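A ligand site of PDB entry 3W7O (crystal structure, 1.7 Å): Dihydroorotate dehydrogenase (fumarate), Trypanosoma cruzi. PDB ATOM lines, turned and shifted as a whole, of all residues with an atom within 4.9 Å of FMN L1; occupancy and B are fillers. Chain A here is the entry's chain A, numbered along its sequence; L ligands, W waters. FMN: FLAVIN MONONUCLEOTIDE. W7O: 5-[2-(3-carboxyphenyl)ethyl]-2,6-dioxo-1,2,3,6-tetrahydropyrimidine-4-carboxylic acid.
N of Thr 273 is in hydrogen-bond range of O3P of FMN L1 (2.8 Å). OG1 of Thr 273 is in hydrogen-bond range of O3P of FMN L1. NZ of Lys 44 is in hydrogen-bond range of O4 of FMN L1. A nitrogen (N3) of FMN L1 sits at hydrogen-bond distance from the side-chain hydroxyl of Ser 45, at 2.7 Å. The backbone NH (N) of Gly 223 lies within hydrogen-bond range of an oxygen (O2P) of FMN L1 (2.7 Å). The backbone NH of Ala 20 lies within hydrogen-bond range of an oxygen (O2') of FMN L1 (3.5 Å). The backbone carbonyl oxygen (O) of Ala 20 is in hydrogen-bond range of an oxygen (O2') of FMN L1 (2.8 Å). N of Gly 251 lies within hydrogen-bond range of O2P of FMN L1. O2' of FMN L1 sits at hydrogen-bond distance from NZ of Lys 165 (2.9 Å). The backbone NH of Gly 272 sits at hydrogen-bond distance from an oxygen (O1P) of FMN L1, at 2.9 Å. An oxygen (O3') of FMN L1 sits at hydrogen-bond distance from the backbone carbonyl oxygen (O) of Val 194, 3.0 Å away. O2 of FMN L1 lies within hydrogen-bond range of ND2 of Asn 195. The side-chain amide nitrogen (ND2) of Asn 128 sits at hydrogen-bond distance from an oxygen (O2) of FMN L1 (3.4 Å). An oxygen (O3') of FMN L1 is in hydrogen-bond range of the side-chain sulfur (SG) of Cys 249 (3.5 Å). The side-chain amino group of Lys 44 lies within salt-bridge range of an oxygen (OAB) of W7O L2, at 3.2 Å. The side-chain amide oxygen (OD1) of Asn 195 is in hydrogen-bond range of a nitrogen (NAN) of W7O L2 (2.8 Å). ND2 of Asn 128 is in hydrogen-bond range of OAD of W7O L2, at 2.9 Å. OD1 of Asn 68 is in hydrogen-bond range of NAM of W7O L2, at 2.9 Å. OAF of W7O L2 is in hydrogen-bond range of N of Met 70 (3.1 Å). An oxygen (OAC) of W7O L2 lies within hydrogen-bond range of the side-chain hydroxyl (OG) of Ser 196, at 2.8 Å. The backbone NH (N) of Leu 72 lies within hydrogen-bond range of an oxygen (OAB) of W7O L2, 2.8 Å away.
A nitrogen (N1) of FMN L1 sits close to a nitrogen (NAN) of W7O L2 (3.4 Å).
The side-chain hydroxyl of Ser 66 is in hydrogen-bond range of the side-chain hydroxyl of Thr 273 (2.7 Å). The backbone NH (N) of Val 194 lies within hydrogen-bond range of the backbone carbonyl oxygen (O) of Cys 249, at 2.9 Å. The side-chain amide nitrogen (ND2) of Asn 195 lies within hydrogen-bond range of the side-chain amide oxygen (OD1) of Asn 128. OG of Ser 196 sits at hydrogen-bond distance from OD1 of Asn 195, at 3.4 Å. The backbone NH of Ala 19 lies within hydrogen-bond range of the backbone carbonyl oxygen of Val 271 (3.0 Å). OD1 of Asn 68 is in hydrogen-bond range of N of Met 70 (3.4 Å). SG of Cys 249 is in hydrogen-bond range of OE1 of Gln 270 (3.7 Å). The backbone NH of Ser 66 lies within hydrogen-bond range of the backbone carbonyl oxygen of Gly 222 (2.9 Å).
Merely in contact with FMN L1: Ala 19, Gly 21, Tyr 59, Asn 68, Met 70, Ser 196, Gly 222, Ile 226 and Gly 250.
Water W1 bridges O4' of FMN L1 (2.6 Å) and OG of Ser 196 (3.5 Å). Water W3 lies within hydrogen-bond range of O1P of FMN L1 (2.7 Å), N of Ala 274 (2.9 Å), O of Val 252 (3.0 Å) and N of Thr 273 (3.5 Å). Water W2 lies within hydrogen-bond range of the side-chain hydroxyl (OG) of Ser 98 (2.6 Å), the side-chain carboxylate (OE1) of Glu 126 (2.7 Å) and an oxygen (O2) of FMN L1 (2.8 Å).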
ATOM      1  N   ALA A  19      12.446 -12.806  30.598  1.00  0.00           N
ATOM      2  CA  ALA A  19      11.922 -13.876  29.844  1.00  0.00           C
ATOM      3  C   ALA A  19      12.681 -13.990  28.498  1.00  0.00           C
ATOM      4  O   ALA A  19      13.097 -12.952  27.923  1.00  0.00           O
ATOM      5  CB  ALA A  19      10.446 -13.565  29.569  1.00  0.00           C
ATOM      6  N   ALA A  20      12.918 -15.192  28.008  1.00  0.00           N
ATOM      7  CA  ALA A  20      13.659 -15.338  26.789  1.00  0.00           C
ATOM      8  C   ALA A  20      13.011 -14.512  25.678  1.00  0.00           C
ATOM      9  O   ALA A  20      11.810 -14.440  25.585  1.00  0.00           O
ATOM     10  CB  ALA A  20      13.754 -16.811  26.355  1.00  0.00           C
ATOM     11  N   GLY A  21      13.852 -13.865  24.918  1.00  0.00           N
ATOM     12  CA  GLY A  21      13.375 -13.029  23.840  1.00  0.00           C
ATOM     13  C   GLY A  21      13.417 -11.569  24.147  1.00  0.00           C
ATOM     14  O   GLY A  21      13.556 -10.758  23.207  1.00  0.00           O
ATOM     15  N   VAL A  22      13.363 -11.213  25.424  1.00  0.00           N
ATOM     16  CA  VAL A  22      13.333  -9.802  25.757  1.00  0.00           C
ATOM     17  C   VAL A  22      14.691  -9.314  26.308  1.00  0.00           C
ATOM     18  O   VAL A  22      15.193  -9.878  27.180  1.00  0.00           O
ATOM     19  CB  VAL A  22      12.197  -9.542  26.739  1.00  0.00           C
ATOM     20  CG1 VAL A  22      12.159  -8.116  27.217  1.00  0.00           C
ATOM     21  CG2 VAL A  22      10.893  -9.954  26.145  1.00  0.00           C
ATOM     22  N   LYS A  44      18.477 -14.943  24.240  1.00  0.00           N
ATOM     23  CA  LYS A  44      17.502 -15.179  23.226  1.00  0.00           C
ATOM     24  C   LYS A  44      17.579 -16.607  22.682  1.00  0.00           C
ATOM     25  O   LYS A  44      18.652 -17.085  22.345  1.00  0.00           O
ATOM     26  CB  LYS A  44      17.799 -14.209  22.090  1.00  0.00           C
ATOM     27  CG  LYS A  44      16.889 -14.378  20.821  1.00  0.00           C
ATOM     28  CD  LYS A  44      15.402 -14.184  21.012  1.00  0.00           C
ATOM     29  CE  LYS A  44      14.528 -14.682  19.835  1.00  0.00           C
ATOM     30  NZ  LYS A  44      12.966 -14.496  19.824  1.00  0.00           N
ATOM     31  N   SER A  45      16.414 -17.236  22.530  1.00  0.00           N
ATOM     32  CA  SER A  45      16.297 -18.556  21.873  1.00  0.00           C
ATOM     33  C   SER A  45      17.029 -18.510  20.579  1.00  0.00           C
ATOM     34  O   SER A  45      16.773 -17.674  19.749  1.00  0.00           O
ATOM     35  CB  SER A  45      14.894 -19.054  21.652  1.00  0.00           C
ATOM     36  OG  SER A  45      14.263 -19.223  22.893  1.00  0.00           O
ATOM     37  N   TYR A  59       6.239  -6.938  16.622  1.00  0.00           N
ATOM     38  CA  TYR A  59       5.875  -6.757  18.034  1.00  0.00           C
ATOM     39  C   TYR A  59       5.134  -5.498  18.243  1.00  0.00           C
ATOM     40  O   TYR A  59       5.537  -4.445  17.736  1.00  0.00           O
ATOM     41  CB  TYR A  59       7.163  -6.759  18.890  1.00  0.00           C
ATOM     42  CG  TYR A  59       6.930  -6.358  20.341  1.00  0.00           C
ATOM     43  CD1 TYR A  59       6.607  -7.311  21.303  1.00  0.00           C
ATOM     44  CD2 TYR A  59       6.985  -5.017  20.806  1.00  0.00           C
ATOM     45  CE1 TYR A  59       6.353  -6.984  22.641  1.00  0.00           C
ATOM     46  CE2 TYR A  59       6.671  -4.679  22.109  1.00  0.00           C
ATOM     47  CZ  TYR A  59       6.429  -5.661  23.074  1.00  0.00           C
ATOM     48  OH  TYR A  59       6.223  -5.317  24.406  1.00  0.00           O
ATOM     49  N   SER A  66       1.034  -7.544  25.110  1.00  0.00           N
ATOM     50  CA  SER A  66       1.736  -7.450  23.854  1.00  0.00           C
ATOM     51  C   SER A  66       1.323  -8.666  22.946  1.00  0.00           C
ATOM     52  O   SER A  66       0.803  -9.670  23.368  1.00  0.00           O
ATOM     53  CB  SER A  66       3.262  -7.488  24.105  1.00  0.00           C
ATOM     54  OG  SER A  66       3.616  -8.826  24.568  1.00  0.00           O
ATOM     55  N   ASN A  68       3.253 -10.743  19.498  1.00  0.00           N
ATOM     56  CA  ASN A  68       4.473 -10.826  18.680  1.00  0.00           C
ATOM     57  C   ASN A  68       4.439 -12.060  17.751  1.00  0.00           C
ATOM     58  O   ASN A  68       4.008 -13.147  18.101  1.00  0.00           O
ATOM     59  CB  ASN A  68       5.726 -10.825  19.549  1.00  0.00           C
ATOM     60  CG  ASN A  68       6.113 -12.208  20.021  1.00  0.00           C
ATOM     61  OD1 ASN A  68       6.738 -13.009  19.289  1.00  0.00           O
ATOM     62  ND2 ASN A  68       5.753 -12.489  21.214  1.00  0.00           N
ATOM     63  N   MET A  70       7.786 -12.716  16.096  1.00  0.00           N
ATOM     64  CA  MET A  70       9.095 -12.230  15.777  1.00  0.00           C
ATOM     65  C   MET A  70       9.772 -13.106  14.711  1.00  0.00           C
ATOM     66  O   MET A  70      10.606 -12.622  13.923  1.00  0.00           O
ATOM     67  CB  MET A  70       9.953 -12.286  17.005  1.00  0.00           C
ATOM     68  CG  MET A  70       9.562 -11.477  18.231  1.00  0.00           C
ATOM     69  SD  MET A  70       9.334  -9.754  17.882  1.00  0.00           S
ATOM     70  CE  MET A  70      11.005  -9.203  17.785  1.00  0.00           C
ATOM     71  N   LEU A  72      11.762 -15.818  15.476  1.00  0.00           N
ATOM     72  CA  LEU A  72      12.999 -16.312  15.991  1.00  0.00           C
ATOM     73  C   LEU A  72      14.250 -15.619  15.401  1.00  0.00           C
ATOM     74  O   LEU A  72      15.329 -16.232  15.078  1.00  0.00           O
ATOM     75  CB  LEU A  72      13.042 -17.832  15.819  1.00  0.00           C
ATOM     76  CG  LEU A  72      13.773 -18.763  16.726  1.00  0.00           C
ATOM     77  CD1 LEU A  72      13.802 -18.418  18.175  1.00  0.00           C
ATOM     78  CD2 LEU A  72      13.257 -20.189  16.386  1.00  0.00           C
ATOM     79  N   SER A  98      18.993 -20.157  26.151  1.00  0.00           N
ATOM     80  CA  SER A  98      17.763 -20.733  25.574  1.00  0.00           C
ATOM     81  C   SER A  98      18.026 -21.216  24.141  1.00  0.00           C
ATOM     82  O   SER A  98      18.689 -20.496  23.382  1.00  0.00           O
ATOM     83  CB  SER A  98      16.632 -19.724  25.535  1.00  0.00           C
ATOM     84  OG  SER A  98      15.535 -20.351  24.841  1.00  0.00           O
ATOM     85  N   GLU A 126      17.965 -23.757  28.899  1.00  0.00           N
ATOM     86  CA  GLU A 126      16.484 -23.713  28.822  1.00  0.00           C
ATOM     87  C   GLU A 126      16.119 -24.113  27.368  1.00  0.00           C
ATOM     88  O   GLU A 126      16.336 -23.388  26.416  1.00  0.00           O
ATOM     89  CB  GLU A 126      15.830 -22.352  29.248  1.00  0.00           C
ATOM     90  CG  GLU A 126      14.306 -22.355  29.225  1.00  0.00           C
ATOM     91  CD  GLU A 126      13.760 -20.988  29.681  1.00  0.00           C
ATOM     92  OE1 GLU A 126      13.589 -20.102  28.794  1.00  0.00           O
ATOM     93  OE2 GLU A 126      13.426 -20.807  30.860  1.00  0.00           O
ATOM     94  N   ASN A 128      13.499 -24.564  24.469  1.00  0.00           N
ATOM     95  CA  ASN A 128      12.187 -24.047  24.170  1.00  0.00           C
ATOM     96  C   ASN A 128      11.425 -25.072  23.319  1.00  0.00           C
ATOM     97  O   ASN A 128      11.743 -25.310  22.142  1.00  0.00           O
ATOM     98  CB  ASN A 128      12.380 -22.769  23.346  1.00  0.00           C
ATOM     99  CG  ASN A 128      11.072 -22.085  23.015  1.00  0.00           C
ATOM    100  OD1 ASN A 128      10.064 -22.440  23.458  1.00  0.00           O
ATOM    101  ND2 ASN A 128      11.212 -20.992  22.312  1.00  0.00           N
ATOM    102  N   LYS A 165      11.024 -24.756  28.401  1.00  0.00           N
ATOM    103  CA  LYS A 165      10.060 -23.638  28.337  1.00  0.00           C
ATOM    104  C   LYS A 165       8.799 -24.176  27.663  1.00  0.00           C
ATOM    105  O   LYS A 165       8.825 -24.674  26.538  1.00  0.00           O
ATOM    106  CB  LYS A 165      10.659 -22.540  27.469  1.00  0.00           C
ATOM    107  CG  LYS A 165       9.777 -21.340  27.246  1.00  0.00           C
ATOM    108  CD  LYS A 165       9.590 -20.488  28.508  1.00  0.00           C
ATOM    109  CE  LYS A 165       8.946 -19.143  28.214  1.00  0.00           C
ATOM    110  NZ  LYS A 165       9.814 -18.194  27.566  1.00  0.00           N
ATOM    111  N   VAL A 194       4.853 -19.693  31.603  1.00  0.00           N
ATOM    112  CA  VAL A 194       4.574 -20.172  30.277  1.00  0.00           C
ATOM    113  C   VAL A 194       5.143 -19.245  29.213  1.00  0.00           C
ATOM    114  O   VAL A 194       5.474 -18.169  29.474  1.00  0.00           O
ATOM    115  CB  VAL A 194       3.065 -20.175  30.023  1.00  0.00           C
ATOM    116  CG1 VAL A 194       2.394 -21.152  30.954  1.00  0.00           C
ATOM    117  CG2 VAL A 194       2.517 -18.812  30.302  1.00  0.00           C
ATOM    118  N   ASN A 195       5.247 -19.786  28.024  1.00  0.00           N
ATOM    119  CA  ASN A 195       5.453 -19.018  26.807  1.00  0.00           C
ATOM    120  C   ASN A 195       4.131 -18.289  26.442  1.00  0.00           C
ATOM    121  O   ASN A 195       3.205 -18.376  27.147  1.00  0.00           O
ATOM    122  CB  ASN A 195       5.899 -19.971  25.678  1.00  0.00           C
ATOM    123  CG  ASN A 195       6.824 -19.313  24.669  1.00  0.00           C
ATOM    124  OD1 ASN A 195       6.580 -18.264  24.269  1.00  0.00           O
ATOM    125  ND2 ASN A 195       7.878 -19.974  24.329  1.00  0.00           N
ATOM    126  N   SER A 196       4.160 -17.525  25.363  1.00  0.00           N
ATOM    127  CA  SER A 196       2.989 -16.709  25.049  1.00  0.00           C
ATOM    128  C   SER A 196       1.762 -17.554  24.808  1.00  0.00           C
ATOM    129  O   SER A 196       1.857 -18.677  24.471  1.00  0.00           O
ATOM    130  CB  SER A 196       3.170 -15.837  23.816  1.00  0.00           C
ATOM    131  OG  SER A 196       4.081 -16.270  22.977  1.00  0.00           O
ATOM    132  N   GLY A 222       1.287 -11.807  25.387  1.00  0.00           N
ATOM    133  CA  GLY A 222       1.946 -11.621  26.649  1.00  0.00           C
ATOM    134  C   GLY A 222       1.320 -10.537  27.458  1.00  0.00           C
ATOM    135  O   GLY A 222       0.477  -9.768  26.948  1.00  0.00           O
ATOM    136  N   GLY A 223       1.662 -10.461  28.721  1.00  0.00           N
ATOM    137  CA  GLY A 223       1.297  -9.363  29.518  1.00  0.00           C
ATOM    138  C   GLY A 223       0.070  -9.604  30.434  1.00  0.00           C
ATOM    139  O   GLY A 223      -0.242 -10.733  30.801  1.00  0.00           O
ATOM    140  N   ILE A 226      -2.526 -12.510  30.190  1.00  0.00           N
ATOM    141  CA  ILE A 226      -2.213 -13.914  30.438  1.00  0.00           C
ATOM    142  C   ILE A 226      -1.853 -14.359  31.886  1.00  0.00           C
ATOM    143  O   ILE A 226      -1.523 -15.457  32.081  1.00  0.00           O
ATOM    144  CB  ILE A 226      -1.108 -14.443  29.472  1.00  0.00           C
ATOM    145  CG1 ILE A 226       0.279 -14.032  29.898  1.00  0.00           C
ATOM    146  CG2 ILE A 226      -1.322 -13.943  28.071  1.00  0.00           C
ATOM    147  CD1 ILE A 226       1.407 -14.778  29.224  1.00  0.00           C
ATOM    148  N   CYS A 249       6.462 -17.514  34.399  1.00  0.00           N
ATOM    149  CA  CYS A 249       6.572 -16.454  33.379  1.00  0.00           C
ATOM    150  C   CYS A 249       5.162 -16.141  32.876  1.00  0.00           C
ATOM    151  O   CYS A 249       4.409 -17.059  32.605  1.00  0.00           O
ATOM    152  CB  CYS A 249       7.450 -16.925  32.260  1.00  0.00           C
ATOM    153  SG  CYS A 249       7.814 -15.664  31.036  1.00  0.00           S
ATOM    154  N   GLY A 250       4.785 -14.877  32.876  1.00  0.00           N
ATOM    155  CA  GLY A 250       3.573 -14.400  32.274  1.00  0.00           C
ATOM    156  C   GLY A 250       2.838 -13.425  33.118  1.00  0.00           C
ATOM    157  O   GLY A 250       2.433 -13.726  34.246  1.00  0.00           O
ATOM    158  N   GLY A 251       2.636 -12.243  32.562  1.00  0.00           N
ATOM    159  CA  GLY A 251       1.856 -11.235  33.293  1.00  0.00           C
ATOM    160  C   GLY A 251       2.502 -10.607  34.453  1.00  0.00           C
ATOM    161  O   GLY A 251       1.776  -9.998  35.215  1.00  0.00           O
ATOM    162  N   VAL A 252       3.814 -10.688  34.615  1.00  0.00           N
ATOM    163  CA  VAL A 252       4.401 -10.018  35.798  1.00  0.00           C
ATOM    164  C   VAL A 252       4.722  -8.589  35.468  1.00  0.00           C
ATOM    165  O   VAL A 252       5.582  -8.335  34.638  1.00  0.00           O
ATOM    166  CB  VAL A 252       5.688 -10.744  36.306  1.00  0.00           C
ATOM    167  CG1 VAL A 252       6.376  -9.989  37.406  1.00  0.00           C
ATOM    168  CG2 VAL A 252       5.385 -12.161  36.715  1.00  0.00           C
ATOM    169  N   GLN A 270      10.140 -14.872  35.705  1.00  0.00           N
ATOM    170  CA  GLN A 270      10.653 -14.180  34.519  1.00  0.00           C
ATOM    171  C   GLN A 270       9.683 -13.058  34.104  1.00  0.00           C
ATOM    172  O   GLN A 270       8.440 -13.176  34.329  1.00  0.00           O
ATOM    173  CB  GLN A 270      10.748 -15.184  33.372  1.00  0.00           C
ATOM    174  CG  GLN A 270      11.490 -16.468  33.743  1.00  0.00           C
ATOM    175  CD  GLN A 270      11.784 -17.360  32.546  1.00  0.00           C
ATOM    176  OE1 GLN A 270      11.089 -17.326  31.531  1.00  0.00           O
ATOM    177  NE2 GLN A 270      12.818 -18.189  32.684  1.00  0.00           N
ATOM    178  N   VAL A 271      10.224 -12.051  33.442  1.00  0.00           N
ATOM    179  CA  VAL A 271       9.535 -10.859  33.090  1.00  0.00           C
ATOM    180  C   VAL A 271       9.801 -10.582  31.606  1.00  0.00           C
ATOM    181  O   VAL A 271      10.956 -10.333  31.205  1.00  0.00           O
ATOM    182  CB  VAL A 271       9.999  -9.682  33.970  1.00  0.00           C
ATOM    183  CG1 VAL A 271       9.142  -8.472  33.702  1.00  0.00           C
ATOM    184  CG2 VAL A 271       9.998 -10.108  35.468  1.00  0.00           C
ATOM    185  N   GLY A 272       8.723 -10.594  30.792  1.00  0.00           N
ATOM    186  CA  GLY A 272       8.771 -10.401  29.341  1.00  0.00           C
ATOM    187  C   GLY A 272       8.248  -9.004  28.995  1.00  0.00           C
ATOM    188  O   GLY A 272       8.979  -7.999  29.027  1.00  0.00           O
ATOM    189  N   THR A 273       6.955  -8.939  28.640  1.00  0.00           N
ATOM    190  CA  THR A 273       6.307  -7.730  28.175  1.00  0.00           C
ATOM    191  C   THR A 273       6.628  -6.530  29.078  1.00  0.00           C
ATOM    192  O   THR A 273       6.999  -5.501  28.573  1.00  0.00           O
ATOM    193  CB  THR A 273       4.794  -7.953  28.084  1.00  0.00           C
ATOM    194  OG1 THR A 273       4.514  -9.019  27.125  1.00  0.00           O
ATOM    195  CG2 THR A 273       4.081  -6.716  27.645  1.00  0.00           C
ATOM    196  N   ALA A 274       6.535  -6.703  30.396  1.00  0.00           N
ATOM    197  CA  ALA A 274       6.687  -5.536  31.272  1.00  0.00           C
ATOM    198  C   ALA A 274       8.094  -4.957  31.219  1.00  0.00           C
ATOM    199  O   ALA A 274       8.306  -3.787  31.285  1.00  0.00           O
ATOM    200  CB  ALA A 274       6.299  -5.910  32.682  1.00  0.00           C
HETATM  201  N1  FMN L   1      10.040 -17.141  24.570  1.00  0.00           N
HETATM  202  C2  FMN L   1      10.997 -18.025  24.278  1.00  0.00           C
HETATM  203  O2  FMN L   1      11.116 -19.029  25.046  1.00  0.00           O
HETATM  204  N3  FMN L   1      11.997 -17.792  23.365  1.00  0.00           N
HETATM  205  C4  FMN L   1      12.032 -16.616  22.706  1.00  0.00           C
HETATM  206  O4  FMN L   1      12.892 -16.332  21.804  1.00  0.00           O
HETATM  207  C4A FMN L   1      10.954 -15.632  22.920  1.00  0.00           C
HETATM  208  N5  FMN L   1      10.952 -14.478  22.202  1.00  0.00           N
HETATM  209  C5A FMN L   1      10.033 -13.513  22.569  1.00  0.00           C
HETATM  210  C6  FMN L   1      10.160 -12.205  22.001  1.00  0.00           C
HETATM  211  C7  FMN L   1       9.243 -11.263  22.343  1.00  0.00           C
HETATM  212  C7M FMN L   1       9.317  -9.882  21.719  1.00  0.00           C
HETATM  213  C8  FMN L   1       8.258 -11.518  23.362  1.00  0.00           C
HETATM  214  C8M FMN L   1       7.258 -10.424  23.743  1.00  0.00           C
HETATM  215  C9  FMN L   1       8.187 -12.771  23.992  1.00  0.00           C
HETATM  216  C9A FMN L   1       9.065 -13.777  23.613  1.00  0.00           C
HETATM  217  N10 FMN L   1       9.007 -15.046  24.205  1.00  0.00           N
HETATM  218  C10 FMN L   1       9.953 -15.956  23.919  1.00  0.00           C
HETATM  219  C1' FMN L   1       8.038 -15.365  25.249  1.00  0.00           C
HETATM  220  C2' FMN L   1       8.410 -14.746  26.570  1.00  0.00           C
HETATM  221  O2' FMN L   1       9.584 -15.396  26.981  1.00  0.00           O
HETATM  222  C3' FMN L   1       7.329 -14.995  27.531  1.00  0.00           C
HETATM  223  O3' FMN L   1       7.199 -16.427  27.718  1.00  0.00           O
HETATM  224  C4' FMN L   1       5.944 -14.421  27.162  1.00  0.00           C
HETATM  225  O4' FMN L   1       6.150 -13.123  26.606  1.00  0.00           O
HETATM  226  C5' FMN L   1       5.061 -14.312  28.449  1.00  0.00           C
HETATM  227  O5' FMN L   1       5.558 -13.461  29.491  1.00  0.00           O
HETATM  228  P   FMN L   1       5.082 -11.946  29.679  1.00  0.00           P
HETATM  229  O1P FMN L   1       5.970 -11.418  30.783  1.00  0.00           O
HETATM  230  O2P FMN L   1       3.593 -12.002  29.923  1.00  0.00           O
HETATM  231  O3P FMN L   1       5.381 -11.259  28.336  1.00  0.00           O
HETATM  232  OAA W7O L   2       9.123 -18.659  13.966  1.00  0.00           O
HETATM  233  CAO W7O L   2       7.957 -18.661  14.476  1.00  0.00           C
HETATM  234  OAE W7O L   2       6.907 -18.622  13.727  1.00  0.00           O
HETATM  235  CAR W7O L   2       7.772 -18.897  15.824  1.00  0.00           C
HETATM  236  CAJ W7O L   2       8.910 -19.130  16.662  1.00  0.00           C
HETATM  237  CAI W7O L   2       6.461 -18.892  16.289  1.00  0.00           C
HETATM  238  CAG W7O L   2       6.167 -19.124  17.610  1.00  0.00           C
HETATM  239  CAH W7O L   2       7.279 -19.371  18.476  1.00  0.00           C
HETATM  240  CAQ W7O L   2       8.627 -19.388  17.994  1.00  0.00           C
HETATM  241  CAK W7O L   2       9.661 -19.566  18.865  1.00  0.00           C
HETATM  242  CAL W7O L   2      10.293 -18.248  19.433  1.00  0.00           C
HETATM  243  CAS W7O L   2       9.338 -17.438  20.139  1.00  0.00           C
HETATM  244  CAV W7O L   2       8.798 -17.899  21.368  1.00  0.00           C
HETATM  245  OAD W7O L   2       9.178 -18.956  21.889  1.00  0.00           O
HETATM  246  NAN W7O L   2       7.846 -17.092  22.003  1.00  0.00           N
HETATM  247  CAU W7O L   2       7.331 -15.924  21.425  1.00  0.00           C
HETATM  248  OAC W7O L   2       6.453 -15.255  21.989  1.00  0.00           O
HETATM  249  NAM W7O L   2       7.936 -15.524  20.226  1.00  0.00           N
HETATM  250  CAT W7O L   2       8.910 -16.259  19.603  1.00  0.00           C
HETATM  251  CAP W7O L   2       9.327 -15.697  18.266  1.00  0.00           C
HETATM  252  OAF W7O L   2       8.335 -15.432  17.534  1.00  0.00           O
HETATM  253  OAB W7O L   2      10.512 -15.536  17.980  1.00  0.00           O
HETATM  254  O   HOH W   1       4.562 -13.200  24.580  1.00  0.00           O
HETATM  255  O   HOH W   2      13.239 -20.557  26.143  1.00  0.00           O
HETATM  256  O   HOH W   3       5.438  -8.987  31.764  1.00  0.00           O
HETATM  257  O   HOH W   4       6.037 -12.372  33.332  1.00  0.00           O
